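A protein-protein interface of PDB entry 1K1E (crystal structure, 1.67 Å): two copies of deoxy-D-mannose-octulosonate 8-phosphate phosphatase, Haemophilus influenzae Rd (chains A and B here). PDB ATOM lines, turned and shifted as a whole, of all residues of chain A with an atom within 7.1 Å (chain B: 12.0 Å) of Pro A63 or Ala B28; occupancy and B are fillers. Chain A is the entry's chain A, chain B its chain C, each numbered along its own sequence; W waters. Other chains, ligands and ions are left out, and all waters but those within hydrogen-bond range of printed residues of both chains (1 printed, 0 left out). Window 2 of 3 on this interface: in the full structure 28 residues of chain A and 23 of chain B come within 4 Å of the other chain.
The guanidinium group (NH1) of Arg A68 lies within hydrogen-bond range of the side-chain hydroxyl (OH) of Tyr B26. The backbone carbonyl oxygen of Asn B29 is in hydrogen-bond range of the guanidinium group of Arg A67, 3.2 Å away. The backbone carbonyl oxygen (O) of Lys A34 is in hydrogen-bond range of the backbone NH (N) of Tyr B26, at 2.9 Å. The backbone carbonyl oxygen (O) of Lys A34 lies close to the backbone carbonyl oxygen (O) of Leu B24 (3.4 Å).
NH2 of Arg B60 sits at hydrogen-bond distance from OH of Tyr B26, at 3.4 Å. OG of Ser A62 sits close to N of Ile A64, 3.1 Å away. N of Ala B32 sits at hydrogen-bond distance from O of His B25 (2.6 Å). The backbone carbonyl oxygen (O) of His B25 sits at hydrogen-bond distance from the backbone NH (N) of Ile B33. The backbone NH (N) of Asn B29 sits at hydrogen-bond distance from the side-chain carboxylate (OD2) of Asp B27 (2.9 Å).
Among the printed residues, merely in contact across the chains: Ala A32 with Asp B27 (3.8 Å), Ile A33 with His B25 (3.8 Å), Ile A33 with Tyr B26 (3.2 Å), Ile A33 with Ile B33 (3.0 Å), Lys A34 with His B25 (3.8 Å), Pro A63 with Ala B28 (3.9 Å), Ile A64 with Tyr B26 (3.5 Å), Ile A64 with Asp B27 (3.8 Å), Ile A64 with Ala B28 (3.7 Å), Arg A67 with Ala B28 (3.4 Å), Arg A67 with Gly B30 (3.6 Å) and Arg A68 with Leu B24 (3.7 Å).
No residue of chain B comes within 4 Å of Asp A61. No residue of chain B comes within 4 Å of Ser A62. Of chain B, only Ala B28 (3.9 Å) comes within 4 Å of Pro A63. No residue of chain B comes within 4 Å of Leu A65. Of the printed residues of chain A, Tyr B26 touches Ile A33, Lys A34, Ile A64 and Arg A68. Ala B28 touches just these residues of chain A: Pro A63, Ile A64 and Arg A67. Of the printed residues of chain A, Gly B30 touches Arg A67. The nearest residue of chain B that does not touch Pro A63 is Asp B27 (5.0 Å). The nearest residue of chain A that does not touch Ala B28 is Ala A32 (5.6 Å). The nearest printed residue of chain A that does not touch Leu B24 is Ile A33 (5.9 Å).
Of the 12 printed residues of chain A, 7 touch a printed residue of chain B. Hydrophobic or aromatic side chains of chain A within 4 Å of the printed part of chain B: Ile A33, Pro A63 and Ile A64. Of the 12 printed residues of chain B, 8 touch a printed residue of chain A. Hydrophobic or aromatic side chains of chain B that line the printed part of chain A: Leu B24, His B25, Tyr B26, Ala B28 and Ile B33. Among the printed residues, 16 pairs touch across the chains.
Ile A33 touches its own counterpart, Ile B33. Positions printed for both chains: 32, 33 and 64.
Water W1 lies within hydrogen-bond range of the guanidinium group of Arg A67 (2.6 Å) and the backbone carbonyl oxygen of Ala B28 (3.0 Å).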
ATOM      1  N   ALA A  32     -10.035   0.183 -14.661  1.00  0.00           N
ATOM      2  CA  ALA A  32      -8.860   0.594 -15.407  1.00  0.00           C
ATOM      3  C   ALA A  32      -8.845   2.061 -15.677  1.00  0.00           C
ATOM      4  O   ALA A  32      -7.797   2.629 -15.904  1.00  0.00           O
ATOM      5  CB  ALA A  32      -8.793  -0.162 -16.714  1.00  0.00           C
ATOM      6  N   ILE A  33     -10.017   2.670 -15.664  1.00  0.00           N
ATOM      7  CA  ILE A  33     -10.202   4.085 -15.937  1.00  0.00           C
ATOM      8  C   ILE A  33     -11.332   4.527 -15.018  1.00  0.00           C
ATOM      9  O   ILE A  33     -12.271   3.741 -14.745  1.00  0.00           O
ATOM     10  CB  ILE A  33     -10.705   4.310 -17.415  1.00  0.00           C
ATOM     11  CG1 ILE A  33      -9.585   4.052 -18.425  1.00  0.00           C
ATOM     12  CG2 ILE A  33     -11.209   5.780 -17.624  1.00  0.00           C
ATOM     13  CD1 ILE A  33     -10.150   3.872 -19.792  1.00  0.00           C
ATOM     14  N   LYS A  34     -11.150   5.699 -14.443  1.00  0.00           N
ATOM     15  CA  LYS A  34     -12.215   6.366 -13.706  1.00  0.00           C
ATOM     16  C   LYS A  34     -12.469   7.668 -14.426  1.00  0.00           C
ATOM     17  O   LYS A  34     -11.536   8.418 -14.714  1.00  0.00           O
ATOM     18  CB  LYS A  34     -11.877   6.599 -12.235  1.00  0.00           C
ATOM     19  CG  LYS A  34     -11.789   5.277 -11.503  1.00  0.00           C
ATOM     20  CD  LYS A  34     -11.759   5.490  -9.974  1.00  0.00           C
ATOM     21  CE  LYS A  34     -13.184   5.871  -9.505  1.00  0.00           C
ATOM     22  NZ  LYS A  34     -14.249   4.752  -9.731  1.00  0.00           N
ATOM     23  N   ASP A  61     -11.113   1.841  -2.941  1.00  0.00           N
ATOM     24  CA  ASP A  61      -9.841   2.570  -2.904  1.00  0.00           C
ATOM     25  C   ASP A  61      -9.073   2.173  -4.163  1.00  0.00           C
ATOM     26  O   ASP A  61      -9.035   1.013  -4.499  1.00  0.00           O
ATOM     27  CB  ASP A  61      -9.039   2.117  -1.674  1.00  0.00           C
ATOM     28  CG  ASP A  61      -7.840   3.034  -1.360  1.00  0.00           C
ATOM     29  OD1 ASP A  61      -7.207   2.865  -0.278  1.00  0.00           O
ATOM     30  OD2 ASP A  61      -7.518   3.936  -2.162  1.00  0.00           O
ATOM     31  N   SER A  62      -8.504   3.125  -4.890  1.00  0.00           N
ATOM     32  CA  SER A  62      -7.707   2.744  -6.040  1.00  0.00           C
ATOM     33  C   SER A  62      -6.686   3.819  -6.253  1.00  0.00           C
ATOM     34  O   SER A  62      -6.855   4.953  -5.852  1.00  0.00           O
ATOM     35  CB  SER A  62      -8.543   2.579  -7.307  1.00  0.00           C
ATOM     36  OG  SER A  62      -8.756   3.824  -7.922  1.00  0.00           O
ATOM     37  N   PRO A  63      -5.587   3.464  -6.913  1.00  0.00           N
ATOM     38  CA  PRO A  63      -4.562   4.455  -7.150  1.00  0.00           C
ATOM     39  C   PRO A  63      -5.087   5.441  -8.204  1.00  0.00           C
ATOM     40  O   PRO A  63      -4.581   6.562  -8.308  1.00  0.00           O
ATOM     41  CB  PRO A  63      -3.354   3.584  -7.577  1.00  0.00           C
ATOM     42  CG  PRO A  63      -3.967   2.390  -8.130  1.00  0.00           C
ATOM     43  CD  PRO A  63      -5.122   2.107  -7.264  1.00  0.00           C
ATOM     44  N   ILE A  64      -6.123   5.050  -8.951  1.00  0.00           N
ATOM     45  CA  ILE A  64      -6.731   6.007  -9.916  1.00  0.00           C
ATOM     46  C   ILE A  64      -7.443   7.100  -9.113  1.00  0.00           C
ATOM     47  O   ILE A  64      -7.260   8.277  -9.331  1.00  0.00           O
ATOM     48  CB  ILE A  64      -7.759   5.335 -10.848  1.00  0.00           C
ATOM     49  CG1 ILE A  64      -7.091   4.202 -11.619  1.00  0.00           C
ATOM     50  CG2 ILE A  64      -8.296   6.414 -11.816  1.00  0.00           C
ATOM     51  CD1 ILE A  64      -8.022   3.344 -12.497  1.00  0.00           C
ATOM     52  N   LEU A  65      -8.299   6.690  -8.203  1.00  0.00           N
ATOM     53  CA  LEU A  65      -8.974   7.658  -7.355  1.00  0.00           C
ATOM     54  C   LEU A  65      -7.977   8.509  -6.565  1.00  0.00           C
ATOM     55  O   LEU A  65      -8.165   9.689  -6.401  1.00  0.00           O
ATOM     56  CB  LEU A  65      -9.986   6.919  -6.424  1.00  0.00           C
ATOM     57  CG  LEU A  65     -10.806   7.892  -5.559  1.00  0.00           C
ATOM     58  CD1 LEU A  65     -11.533   9.002  -6.341  1.00  0.00           C
ATOM     59  CD2 LEU A  65     -11.826   7.079  -4.821  1.00  0.00           C
ATOM     60  N   ARG A  66      -6.888   7.927  -6.086  1.00  0.00           N
ATOM     61  CA  ARG A  66      -5.921   8.716  -5.350  1.00  0.00           C
ATOM     62  C   ARG A  66      -5.229   9.783  -6.204  1.00  0.00           C
ATOM     63  O   ARG A  66      -4.949  10.872  -5.744  1.00  0.00           O
ATOM     64  CB  ARG A  66      -4.940   7.739  -4.688  1.00  0.00           C
ATOM     65  CG  ARG A  66      -5.595   7.135  -3.417  1.00  0.00           C
ATOM     66  CD  ARG A  66      -4.756   6.036  -2.785  1.00  0.00           C
ATOM     67  NE  ARG A  66      -5.379   5.436  -1.586  1.00  0.00           N
ATOM     68  CZ  ARG A  66      -5.167   5.850  -0.341  1.00  0.00           C
ATOM     69  NH1 ARG A  66      -4.378   6.876  -0.108  1.00  0.00           N
ATOM     70  NH2 ARG A  66      -5.658   5.171   0.695  1.00  0.00           N
ATOM     71  N   ARG A  67      -5.017   9.457  -7.470  1.00  0.00           N
ATOM     72  CA  ARG A  67      -4.388  10.382  -8.392  1.00  0.00           C
ATOM     73  C   ARG A  67      -5.334  11.565  -8.611  1.00  0.00           C
ATOM     74  O   ARG A  67      -4.915  12.711  -8.623  1.00  0.00           O
ATOM     75  CB  ARG A  67      -4.109   9.671  -9.710  1.00  0.00           C
ATOM     76  CG  ARG A  67      -3.471  10.603 -10.821  1.00  0.00           C
ATOM     77  CD  ARG A  67      -2.382  11.426 -10.267  1.00  0.00           C
ATOM     78  NE  ARG A  67      -1.810  12.355 -11.242  1.00  0.00           N
ATOM     79  CZ  ARG A  67      -0.625  12.206 -11.821  1.00  0.00           C
ATOM     80  NH1 ARG A  67       0.118  11.150 -11.502  1.00  0.00           N
ATOM     81  NH2 ARG A  67      -0.181  13.115 -12.720  1.00  0.00           N
ATOM     82  N   ARG A  68      -6.620  11.279  -8.757  1.00  0.00           N
ATOM     83  CA  ARG A  68      -7.598  12.359  -8.965  1.00  0.00           C
ATOM     84  C   ARG A  68      -7.628  13.232  -7.725  1.00  0.00           C
ATOM     85  O   ARG A  68      -7.596  14.461  -7.835  1.00  0.00           O
ATOM     86  CB  ARG A  68      -8.970  11.750  -9.267  1.00  0.00           C
ATOM     87  CG  ARG A  68     -10.162  12.803  -9.555  1.00  0.00           C
ATOM     88  CD  ARG A  68      -9.749  13.869 -10.535  1.00  0.00           C
ATOM     89  NE  ARG A  68     -10.855  14.742 -10.861  1.00  0.00           N
ATOM     90  CZ  ARG A  68     -10.766  15.849 -11.575  1.00  0.00           C
ATOM     91  NH1 ARG A  68      -9.580  16.257 -12.067  1.00  0.00           N
ATOM     92  NH2 ARG A  68     -11.887  16.563 -11.753  1.00  0.00           N
ATOM     93  N   ILE A  69      -7.706  12.611  -6.545  1.00  0.00           N
ATOM     94  CA  ILE A  69      -7.695  13.357  -5.287  1.00  0.00           C
ATOM     95  C   ILE A  69      -6.459  14.287  -5.146  1.00  0.00           C
ATOM     96  O   ILE A  69      -6.572  15.459  -4.764  1.00  0.00           O
ATOM     97  CB  ILE A  69      -7.735  12.390  -4.149  1.00  0.00           C
ATOM     98  CG1 ILE A  69      -9.186  11.854  -4.000  1.00  0.00           C
ATOM     99  CG2 ILE A  69      -7.218  13.063  -2.872  1.00  0.00           C
ATOM    100  CD1 ILE A  69      -9.284  10.685  -3.025  1.00  0.00           C
ATOM    101  N   LEU B  24     -12.966  13.607 -17.661  1.00  0.00           N
ATOM    102  CA  LEU B  24     -11.504  13.472 -17.600  1.00  0.00           C
ATOM    103  C   LEU B  24     -11.328  11.959 -17.316  1.00  0.00           C
ATOM    104  O   LEU B  24     -11.689  11.475 -16.247  1.00  0.00           O
ATOM    105  CB  LEU B  24     -10.986  14.326 -16.465  1.00  0.00           C
ATOM    106  CG  LEU B  24     -11.143  15.832 -16.749  1.00  0.00           C
ATOM    107  CD1 LEU B  24     -10.648  16.694 -15.530  1.00  0.00           C
ATOM    108  CD2 LEU B  24     -10.365  16.203 -18.004  1.00  0.00           C
ATOM    109  N   HIS B  25     -10.795  11.214 -18.292  1.00  0.00           N
ATOM    110  CA  HIS B  25     -10.603   9.779 -18.107  1.00  0.00           C
ATOM    111  C   HIS B  25      -9.236   9.500 -17.549  1.00  0.00           C
ATOM    112  O   HIS B  25      -8.233   9.510 -18.245  1.00  0.00           O
ATOM    113  CB  HIS B  25     -10.755   9.053 -19.404  1.00  0.00           C
ATOM    114  CG  HIS B  25     -12.056   9.331 -20.078  1.00  0.00           C
ATOM    115  ND1 HIS B  25     -13.262   8.949 -19.523  1.00  0.00           N
ATOM    116  CD2 HIS B  25     -12.349   9.940 -21.263  1.00  0.00           C
ATOM    117  CE1 HIS B  25     -14.245   9.294 -20.349  1.00  0.00           C
ATOM    118  NE2 HIS B  25     -13.720   9.897 -21.414  1.00  0.00           N
ATOM    119  N   TYR B  26      -9.249   9.202 -16.256  1.00  0.00           N
ATOM    120  CA  TYR B  26      -8.036   8.948 -15.519  1.00  0.00           C
ATOM    121  C   TYR B  26      -7.578   7.514 -15.374  1.00  0.00           C
ATOM    122  O   TYR B  26      -8.387   6.590 -15.299  1.00  0.00           O
ATOM    123  CB  TYR B  26      -8.186   9.416 -14.062  1.00  0.00           C
ATOM    124  CG  TYR B  26      -7.905  10.809 -13.759  1.00  0.00           C
ATOM    125  CD1 TYR B  26      -8.665  11.842 -14.280  1.00  0.00           C
ATOM    126  CD2 TYR B  26      -6.893  11.125 -12.849  1.00  0.00           C
ATOM    127  CE1 TYR B  26      -8.420  13.162 -13.907  1.00  0.00           C
ATOM    128  CE2 TYR B  26      -6.644  12.435 -12.466  1.00  0.00           C
ATOM    129  CZ  TYR B  26      -7.396  13.452 -12.992  1.00  0.00           C
ATOM    130  OH  TYR B  26      -7.092  14.754 -12.670  1.00  0.00           O
ATOM    131  N   ASP B  27      -6.249   7.349 -15.367  1.00  0.00           N
ATOM    132  CA  ASP B  27      -5.740   6.076 -14.882  1.00  0.00           C
ATOM    133  C   ASP B  27      -4.879   6.509 -13.664  1.00  0.00           C
ATOM    134  O   ASP B  27      -4.967   7.650 -13.218  1.00  0.00           O
ATOM    135  CB  ASP B  27      -4.991   5.215 -15.927  1.00  0.00           C
ATOM    136  CG  ASP B  27      -3.730   5.823 -16.442  1.00  0.00           C
ATOM    137  OD1 ASP B  27      -3.186   5.233 -17.378  1.00  0.00           O
ATOM    138  OD2 ASP B  27      -3.289   6.849 -15.970  1.00  0.00           O
ATOM    139  N   ALA B  28      -4.044   5.647 -13.115  1.00  0.00           N
ATOM    140  CA  ALA B  28      -3.279   6.098 -11.937  1.00  0.00           C
ATOM    141  C   ALA B  28      -2.242   7.173 -12.216  1.00  0.00           C
ATOM    142  O   ALA B  28      -1.693   7.772 -11.282  1.00  0.00           O
ATOM    143  CB  ALA B  28      -2.580   4.862 -11.254  1.00  0.00           C
ATOM    144  N   ASN B  29      -1.960   7.417 -13.495  1.00  0.00           N
ATOM    145  CA  ASN B  29      -0.979   8.438 -13.842  1.00  0.00           C
ATOM    146  C   ASN B  29      -1.535   9.765 -14.324  1.00  0.00           C
ATOM    147  O   ASN B  29      -0.765  10.679 -14.700  1.00  0.00           O
ATOM    148  CB  ASN B  29      -0.026   7.845 -14.887  1.00  0.00           C
ATOM    149  CG  ASN B  29       0.866   6.789 -14.299  1.00  0.00           C
ATOM    150  OD1 ASN B  29       1.001   5.690 -14.836  1.00  0.00           O
ATOM    151  ND2 ASN B  29       1.484   7.126 -13.178  1.00  0.00           N
ATOM    152  N   GLY B  30      -2.866   9.907 -14.303  1.00  0.00           N
ATOM    153  CA  GLY B  30      -3.460  11.136 -14.772  1.00  0.00           C
ATOM    154  C   GLY B  30      -4.371  10.822 -15.935  1.00  0.00           C
ATOM    155  O   GLY B  30      -4.899   9.721 -16.019  1.00  0.00           O
ATOM    156  N   GLU B  31      -4.579  11.787 -16.814  1.00  0.00           N
ATOM    157  CA  GLU B  31      -5.464  11.522 -17.976  1.00  0.00           C
ATOM    158  C   GLU B  31      -4.907  10.367 -18.804  1.00  0.00           C
ATOM    159  O   GLU B  31      -3.736  10.354 -19.202  1.00  0.00           O
ATOM    160  CB  GLU B  31      -5.584  12.787 -18.866  1.00  0.00           C
ATOM    161  CG  GLU B  31      -6.238  13.924 -18.227  1.00  0.00           C
ATOM    162  CD  GLU B  31      -6.484  15.046 -19.255  1.00  0.00           C
ATOM    163  OE1 GLU B  31      -7.497  14.909 -20.034  1.00  0.00           O
ATOM    164  OE2 GLU B  31      -5.646  16.011 -19.309  1.00  0.00           O
ATOM    165  N   ALA B  32      -5.753   9.402 -19.115  1.00  0.00           N
ATOM    166  CA  ALA B  32      -5.320   8.241 -19.849  1.00  0.00           C
ATOM    167  C   ALA B  32      -5.919   8.191 -21.272  1.00  0.00           C
ATOM    168  O   ALA B  32      -5.335   7.570 -22.166  1.00  0.00           O
ATOM    169  CB  ALA B  32      -5.756   6.963 -19.062  1.00  0.00           C
ATOM    170  N   ILE B  33      -7.070   8.852 -21.440  1.00  0.00           N
ATOM    171  CA  ILE B  33      -7.813   8.904 -22.715  1.00  0.00           C
ATOM    172  C   ILE B  33      -8.478  10.283 -22.771  1.00  0.00           C
ATOM    173  O   ILE B  33      -8.831  10.800 -21.725  1.00  0.00           O
ATOM    174  CB  ILE B  33      -9.001   7.852 -22.690  1.00  0.00           C
ATOM    175  CG1 ILE B  33      -8.430   6.428 -22.778  1.00  0.00           C
ATOM    176  CG2 ILE B  33      -9.922   8.036 -23.876  1.00  0.00           C
ATOM    177  CD1 ILE B  33      -9.280   5.457 -22.155  1.00  0.00           C
ATOM    178  N   ARG B  60      -4.937  22.797 -19.444  1.00  0.00           N
ATOM    179  CA  ARG B  60      -4.364  21.478 -19.125  1.00  0.00           C
ATOM    180  C   ARG B  60      -3.511  21.170 -20.380  1.00  0.00           C
ATOM    181  O   ARG B  60      -3.841  21.600 -21.471  1.00  0.00           O
ATOM    182  CB  ARG B  60      -5.493  20.423 -18.934  1.00  0.00           C
ATOM    183  CG  ARG B  60      -6.362  20.605 -17.651  1.00  0.00           C
ATOM    184  CD  ARG B  60      -7.470  19.519 -17.352  1.00  0.00           C
ATOM    185  NE  ARG B  60      -6.991  18.263 -16.765  1.00  0.00           N
ATOM    186  CZ  ARG B  60      -6.587  18.082 -15.493  1.00  0.00           C
ATOM    187  NH1 ARG B  60      -6.588  19.079 -14.603  1.00  0.00           N
ATOM    188  NH2 ARG B  60      -6.175  16.878 -15.113  1.00  0.00           N
ATOM    189  N   ILE B  64      -1.695  13.559 -24.916  1.00  0.00           N
ATOM    190  CA  ILE B  64      -2.916  13.106 -25.613  1.00  0.00           C
ATOM    191  C   ILE B  64      -3.509  14.268 -26.379  1.00  0.00           C
ATOM    192  O   ILE B  64      -3.829  14.155 -27.603  1.00  0.00           O
ATOM    193  CB  ILE B  64      -3.945  12.615 -24.615  1.00  0.00           C
ATOM    194  CG1 ILE B  64      -3.408  11.399 -23.848  1.00  0.00           C
ATOM    195  CG2 ILE B  64      -5.183  12.127 -25.370  1.00  0.00           C
ATOM    196  CD1 ILE B  64      -4.440  10.905 -22.778  1.00  0.00           C
HETATM  197  O   HOH W   1       0.482   9.279  -9.803  1.00  0.00           O
